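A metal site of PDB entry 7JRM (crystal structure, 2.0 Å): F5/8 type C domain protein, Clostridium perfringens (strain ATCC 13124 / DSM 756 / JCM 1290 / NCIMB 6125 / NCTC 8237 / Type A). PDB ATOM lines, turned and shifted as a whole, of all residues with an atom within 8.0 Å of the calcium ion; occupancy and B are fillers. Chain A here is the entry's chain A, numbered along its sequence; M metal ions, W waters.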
ATOM      1  N   HIS A 131      11.891  -0.263  25.972  1.00  0.00           N
ATOM      2  CA  HIS A 131      10.451  -0.028  25.844  1.00  0.00           C
ATOM      3  C   HIS A 131       9.730  -0.977  26.790  1.00  0.00           C
ATOM      4  O   HIS A 131      10.005  -2.171  26.790  1.00  0.00           O
ATOM      5  CB  HIS A 131       9.999  -0.249  24.394  1.00  0.00           C
ATOM      6  CG  HIS A 131       8.641   0.289  24.081  1.00  0.00           C
ATOM      7  ND1 HIS A 131       7.502  -0.145  24.707  1.00  0.00           N
ATOM      8  CD2 HIS A 131       8.243   1.222  23.175  1.00  0.00           C
ATOM      9  CE1 HIS A 131       6.455   0.494  24.226  1.00  0.00           C
ATOM     10  NE2 HIS A 131       6.884   1.332  23.293  1.00  0.00           N
ATOM     11  N   SER A 132       8.820  -0.431  27.592  1.00  0.00           N
ATOM     12  CA  SER A 132       8.041  -1.263  28.501  1.00  0.00           C
ATOM     13  C   SER A 132       7.152  -2.214  27.704  1.00  0.00           C
ATOM     14  O   SER A 132       6.680  -1.885  26.611  1.00  0.00           O
ATOM     15  CB  SER A 132       7.196  -0.394  29.425  1.00  0.00           C
ATOM     16  OG  SER A 132       5.911  -0.162  28.884  1.00  0.00           O
ATOM     17  N   ILE A 152      11.256   9.291  30.251  1.00  0.00           N
ATOM     18  CA  ILE A 152      10.593   9.017  28.976  1.00  0.00           C
ATOM     19  C   ILE A 152      11.404   9.668  27.857  1.00  0.00           C
ATOM     20  O   ILE A 152      11.756  10.851  27.939  1.00  0.00           O
ATOM     21  CB  ILE A 152       9.154   9.550  28.995  1.00  0.00           C
ATOM     22  CG1 ILE A 152       8.318   8.776  30.023  1.00  0.00           C
ATOM     23  CG2 ILE A 152       8.525   9.439  27.616  1.00  0.00           C
ATOM     24  CD1 ILE A 152       7.799   7.445  29.529  1.00  0.00           C
ATOM     25  N   VAL A 161       0.161   9.870  26.180  1.00  0.00           N
ATOM     26  CA  VAL A 161      -0.136   8.804  27.130  1.00  0.00           C
ATOM     27  C   VAL A 161       1.105   8.086  27.657  1.00  0.00           C
ATOM     28  O   VAL A 161       0.961   7.122  28.416  1.00  0.00           O
ATOM     29  CB  VAL A 161      -1.095   7.766  26.509  1.00  0.00           C
ATOM     30  CG1 VAL A 161      -2.391   8.427  26.093  1.00  0.00           C
ATOM     31  CG2 VAL A 161      -0.424   7.081  25.321  1.00  0.00           C
ATOM     32  N   SER A 162       2.303   8.514  27.282  1.00  0.00           N
ATOM     33  CA  SER A 162       3.508   7.822  27.711  1.00  0.00           C
ATOM     34  C   SER A 162       3.656   7.859  29.228  1.00  0.00           C
ATOM     35  O   SER A 162       3.521   8.909  29.851  1.00  0.00           O
ATOM     36  CB  SER A 162       4.734   8.455  27.043  1.00  0.00           C
ATOM     37  OG  SER A 162       4.831   8.070  25.678  1.00  0.00           O
ATOM     38  N   SER A 163       3.923   6.686  29.816  1.00  0.00           N
ATOM     39  CA  SER A 163       4.057   6.554  31.259  1.00  0.00           C
ATOM     40  C   SER A 163       4.714   5.233  31.631  1.00  0.00           C
ATOM     41  O   SER A 163       4.260   4.169  31.207  1.00  0.00           O
ATOM     42  CB  SER A 163       2.691   6.668  31.950  1.00  0.00           C
ATOM     43  OG  SER A 163       1.807   5.683  31.458  1.00  0.00           O
ATOM     44  N   VAL A 164       5.791   5.282  32.430  1.00  0.00           N
ATOM     45  CA  VAL A 164       6.518   4.089  32.844  1.00  0.00           C
ATOM     46  C   VAL A 164       6.905   4.234  34.315  1.00  0.00           C
ATOM     47  O   VAL A 164       6.693   5.268  34.940  1.00  0.00           O
ATOM     48  CB  VAL A 164       7.774   3.835  31.989  1.00  0.00           C
ATOM     49  CG1 VAL A 164       7.398   3.538  30.549  1.00  0.00           C
ATOM     50  CG2 VAL A 164       8.713   5.027  32.060  1.00  0.00           C
ATOM     51  N   LYS A 165       7.480   3.162  34.859  1.00  0.00           N
ATOM     52  CA  LYS A 165       8.099   3.178  36.176  1.00  0.00           C
ATOM     53  C   LYS A 165       9.380   2.362  36.098  1.00  0.00           C
ATOM     54  O   LYS A 165       9.361   1.214  35.641  1.00  0.00           O
ATOM     55  CB  LYS A 165       7.168   2.615  37.254  1.00  0.00           C
ATOM     56  CG  LYS A 165       7.732   2.715  38.657  1.00  0.00           C
ATOM     57  CD  LYS A 165       6.955   1.857  39.640  1.00  0.00           C
ATOM     58  CE  LYS A 165       5.455   2.053  39.485  1.00  0.00           C
ATOM     59  NZ  LYS A 165       4.710   0.771  39.603  1.00  0.00           N
ATOM     60  N   VAL A 180       5.618   6.971  38.921  1.00  0.00           N
ATOM     61  CA  VAL A 180       5.176   6.895  37.537  1.00  0.00           C
ATOM     62  C   VAL A 180       5.677   8.125  36.804  1.00  0.00           C
ATOM     63  O   VAL A 180       5.324   9.267  37.148  1.00  0.00           O
ATOM     64  CB  VAL A 180       3.655   6.775  37.448  1.00  0.00           C
ATOM     65  CG1 VAL A 180       3.175   7.115  36.041  1.00  0.00           C
ATOM     66  CG2 VAL A 180       3.219   5.367  37.830  1.00  0.00           C
ATOM     67  N   MET A 181       6.520   7.919  35.788  1.00  0.00           N
ATOM     68  CA  MET A 181       7.128   9.009  35.046  1.00  0.00           C
ATOM     69  C   MET A 181       6.377   9.215  33.736  1.00  0.00           C
ATOM     70  O   MET A 181       6.108   8.257  33.009  1.00  0.00           O
ATOM     71  CB  MET A 181       8.601   8.705  34.760  1.00  0.00           C
ATOM     72  CG  MET A 181       9.516   9.005  35.945  1.00  0.00           C
ATOM     73  SD  MET A 181      11.261   8.825  35.541  1.00  0.00           S
ATOM     74  CE  MET A 181      11.638  10.494  35.001  1.00  0.00           C
ATOM     75  N   ARG A 182       6.014  10.459  33.460  1.00  0.00           N
ATOM     76  CA  ARG A 182       5.262  10.824  32.281  1.00  0.00           C
ATOM     77  C   ARG A 182       6.141  11.641  31.335  1.00  0.00           C
ATOM     78  O   ARG A 182       7.347  11.798  31.550  1.00  0.00           O
ATOM     79  CB  ARG A 182       3.984  11.566  32.682  1.00  0.00           C
ATOM     80  CG  ARG A 182       3.301  10.954  33.893  1.00  0.00           C
ATOM     81  CD  ARG A 182       1.876  11.456  34.056  1.00  0.00           C
ATOM     82  NE  ARG A 182       1.099  10.585  34.929  1.00  0.00           N
ATOM     83  CZ  ARG A 182       0.422   9.509  34.506  1.00  0.00           C
ATOM     84  NH1 ARG A 182       0.436   9.182  33.222  1.00  0.00           N
ATOM     85  NH2 ARG A 182      -0.250   8.770  35.368  1.00  0.00           N
ATOM     86  N   ASP A 205       8.415  -0.834  33.963  1.00  0.00           N
ATOM     87  CA  ASP A 205       7.029  -1.266  34.008  1.00  0.00           C
ATOM     88  C   ASP A 205       6.140  -0.319  33.205  1.00  0.00           C
ATOM     89  O   ASP A 205       6.553   0.759  32.778  1.00  0.00           O
ATOM     90  CB  ASP A 205       6.547  -1.367  35.459  1.00  0.00           C
ATOM     91  CG  ASP A 205       5.608  -2.530  35.678  1.00  0.00           C
ATOM     92  OD1 ASP A 205       4.905  -2.921  34.716  1.00  0.00           O
ATOM     93  OD2 ASP A 205       5.564  -3.072  36.799  1.00  0.00           O
ATOM     94  N   VAL A 206       4.892  -0.744  33.010  1.00  0.00           N
ATOM     95  CA  VAL A 206       4.015  -0.079  32.050  1.00  0.00           C
ATOM     96  C   VAL A 206       3.182   1.053  32.646  1.00  0.00           C
ATOM     97  O   VAL A 206       2.630   1.858  31.894  1.00  0.00           O
ATOM     98  CB  VAL A 206       3.074  -1.106  31.390  1.00  0.00           C
ATOM     99  CG1 VAL A 206       3.877  -2.177  30.672  1.00  0.00           C
ATOM    100  CG2 VAL A 206       2.151  -1.730  32.428  1.00  0.00           C
ATOM    101  N   ALA A 207       3.074   1.131  33.979  1.00  0.00           N
ATOM    102  CA  ALA A 207       2.270   2.156  34.668  1.00  0.00           C
ATOM    103  C   ALA A 207       0.845   2.082  34.109  1.00  0.00           C
ATOM    104  O   ALA A 207       0.270   0.985  34.062  1.00  0.00           O
ATOM    105  CB  ALA A 207       2.962   3.510  34.543  1.00  0.00           C
ATOM    106  N   ASP A 208       0.252   3.195  33.680  1.00  0.00           N
ATOM    107  CA  ASP A 208      -1.096   3.188  33.123  1.00  0.00           C
ATOM    108  C   ASP A 208      -1.040   3.173  31.595  1.00  0.00           C
ATOM    109  O   ASP A 208       0.017   3.320  30.986  1.00  0.00           O
ATOM    110  CB  ASP A 208      -1.898   4.391  33.628  1.00  0.00           C
ATOM    111  CG  ASP A 208      -1.174   5.707  33.450  1.00  0.00           C
ATOM    112  OD1 ASP A 208      -1.368   6.618  34.290  1.00  0.00           O
ATOM    113  OD2 ASP A 208      -0.413   5.861  32.473  1.00  0.00           O
ATOM    114  N   ASN A 209      -2.224   2.986  30.996  1.00  0.00           N
ATOM    115  CA  ASN A 209      -2.390   2.998  29.546  1.00  0.00           C
ATOM    116  C   ASN A 209      -1.573   1.903  28.853  1.00  0.00           C
ATOM    117  O   ASN A 209      -1.217   2.030  27.677  1.00  0.00           O
ATOM    118  CB  ASN A 209      -2.046   4.370  28.947  1.00  0.00           C
ATOM    119  CG  ASN A 209      -3.179   5.366  29.072  1.00  0.00           C
ATOM    120  OD1 ASN A 209      -3.079   6.343  29.817  1.00  0.00           O
ATOM    121  ND2 ASN A 209      -4.262   5.119  28.354  1.00  0.00           N
ATOM    122  N   GLY A 210      -1.283   0.819  29.573  1.00  0.00           N
ATOM    123  CA  GLY A 210      -0.474  -0.233  28.999  1.00  0.00           C
ATOM    124  C   GLY A 210       0.916   0.265  28.666  1.00  0.00           C
ATOM    125  O   GLY A 210       1.473   1.149  29.335  1.00  0.00           O
ATOM    126  N   ASN A 211       1.494  -0.307  27.607  1.00  0.00           N
ATOM    127  CA  ASN A 211       2.836   0.058  27.165  1.00  0.00           C
ATOM    128  C   ASN A 211       2.817   1.039  25.993  1.00  0.00           C
ATOM    129  O   ASN A 211       3.836   1.202  25.317  1.00  0.00           O
ATOM    130  CB  ASN A 211       3.622  -1.203  26.783  1.00  0.00           C
ATOM    131  CG  ASN A 211       3.069  -1.897  25.550  1.00  0.00           C
ATOM    132  OD1 ASN A 211       1.956  -1.614  25.099  1.00  0.00           O
ATOM    133  ND2 ASN A 211       3.858  -2.807  24.989  1.00  0.00           N
ATOM    134  N   ASN A 212       1.693   1.698  25.757  1.00  0.00           N
ATOM    135  CA  ASN A 212       1.544   2.548  24.576  1.00  0.00           C
ATOM    136  C   ASN A 212       2.523   3.713  24.621  1.00  0.00           C
ATOM    137  O   ASN A 212       2.490   4.537  25.532  1.00  0.00           O
ATOM    138  CB  ASN A 212       0.107   3.060  24.479  1.00  0.00           C
ATOM    139  CG  ASN A 212      -0.246   3.508  23.074  1.00  0.00           C
ATOM    140  OD1 ASN A 212       0.321   3.031  22.097  1.00  0.00           O
ATOM    141  ND2 ASN A 212      -1.187   4.441  22.965  1.00  0.00           N
ATOM    142  N   TRP A 213       3.399   3.768  23.605  1.00  0.00           N
ATOM    143  CA  TRP A 213       4.383   4.845  23.461  1.00  0.00           C
ATOM    144  C   TRP A 213       5.295   4.961  24.672  1.00  0.00           C
ATOM    145  O   TRP A 213       5.725   6.052  25.043  1.00  0.00           O
ATOM    146  CB  TRP A 213       3.697   6.186  23.168  1.00  0.00           C
ATOM    147  CG  TRP A 213       2.845   6.154  21.942  1.00  0.00           C
ATOM    148  CD1 TRP A 213       1.498   6.343  21.871  1.00  0.00           C
ATOM    149  CD2 TRP A 213       3.289   5.926  20.596  1.00  0.00           C
ATOM    150  NE1 TRP A 213       1.068   6.242  20.566  1.00  0.00           N
ATOM    151  CE2 TRP A 213       2.150   5.989  19.767  1.00  0.00           C
ATOM    152  CE3 TRP A 213       4.529   5.667  20.010  1.00  0.00           C
ATOM    153  CZ2 TRP A 213       2.219   5.800  18.391  1.00  0.00           C
ATOM    154  CZ3 TRP A 213       4.603   5.487  18.643  1.00  0.00           C
ATOM    155  CH2 TRP A 213       3.447   5.559  17.845  1.00  0.00           C
ATOM    156  N   ASP A 214       5.622   3.826  25.287  1.00  0.00           N
ATOM    157  CA  ASP A 214       6.450   3.795  26.490  1.00  0.00           C
ATOM    158  C   ASP A 214       7.934   3.668  26.119  1.00  0.00           C
ATOM    159  O   ASP A 214       8.606   2.686  26.429  1.00  0.00           O
ATOM    160  CB  ASP A 214       6.012   2.666  27.406  1.00  0.00           C
ATOM    161  CG  ASP A 214       4.827   3.039  28.281  1.00  0.00           C
ATOM    162  OD1 ASP A 214       4.361   4.192  28.180  1.00  0.00           O
ATOM    163  OD2 ASP A 214       4.373   2.178  29.061  1.00  0.00           O
ATOM    164  N   HIS A 215       8.437   4.699  25.455  1.00  0.00           N
ATOM    165  CA  HIS A 215       9.859   4.786  25.134  1.00  0.00           C
ATOM    166  C   HIS A 215      10.617   5.226  26.382  1.00  0.00           C
ATOM    167  O   HIS A 215      10.415   6.344  26.865  1.00  0.00           O
ATOM    168  CB  HIS A 215      10.106   5.749  23.976  1.00  0.00           C
ATOM    169  CG  HIS A 215       9.522   5.294  22.673  1.00  0.00           C
ATOM    170  ND1 HIS A 215       9.984   5.765  21.457  1.00  0.00           N
ATOM    171  CD2 HIS A 215       8.529   4.421  22.389  1.00  0.00           C
ATOM    172  CE1 HIS A 215       9.293   5.195  20.488  1.00  0.00           C
ATOM    173  NE2 HIS A 215       8.400   4.376  21.023  1.00  0.00           N
HETATM  174 CA    CA M   1       2.399   3.282  30.026  1.00  0.00          CA
HETATM  175  O   HOH W   1       1.350   4.244  28.085  1.00  0.00           O
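The backbone carbonyl oxygen (O) of Val 206 binds the calcium ion, at 2.4 Å. The calcium ion is bound by O of Ser 163 (2.4 Å). The calcium ion is bound by water W1, 2.4 Å away. The calcium ion is bound by O of Gly 210 (2.4 Å). OD2 of Asp 214 is bound to the calcium ion (2.5 Å). The calcium ion is bound by O of Asp 208 (2.6 Å). The side-chain carboxylate (OD1) of Asp 214 is bound to the calcium ion (2.8 Å). OG of Ser 163 binds the calcium ion, at 2.9 Å.
The backbone carbonyl oxygen (O) of Val 161 sits close to the side-chain hydroxyl (OG) of Ser 163. The backbone NH of Ser 132 lies within hydrogen-bond range of the backbone carbonyl oxygen of Asp 214, at 3.3 Å. The backbone NH of Asp 214 sits at hydrogen-bond distance from a ring nitrogen (NE2) of His 131 (3.4 Å). OD1 of Asp 208 lies within salt-bridge range of NH2 of Arg 182 (2.7 Å).
Within 4 Å of the calcium ion: Ser 163, Val 206, Asp 208, Gly 210 and Asp 214. The nearest printed residue that does not touch the calcium ion is Asn 211 (4.3 Å).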
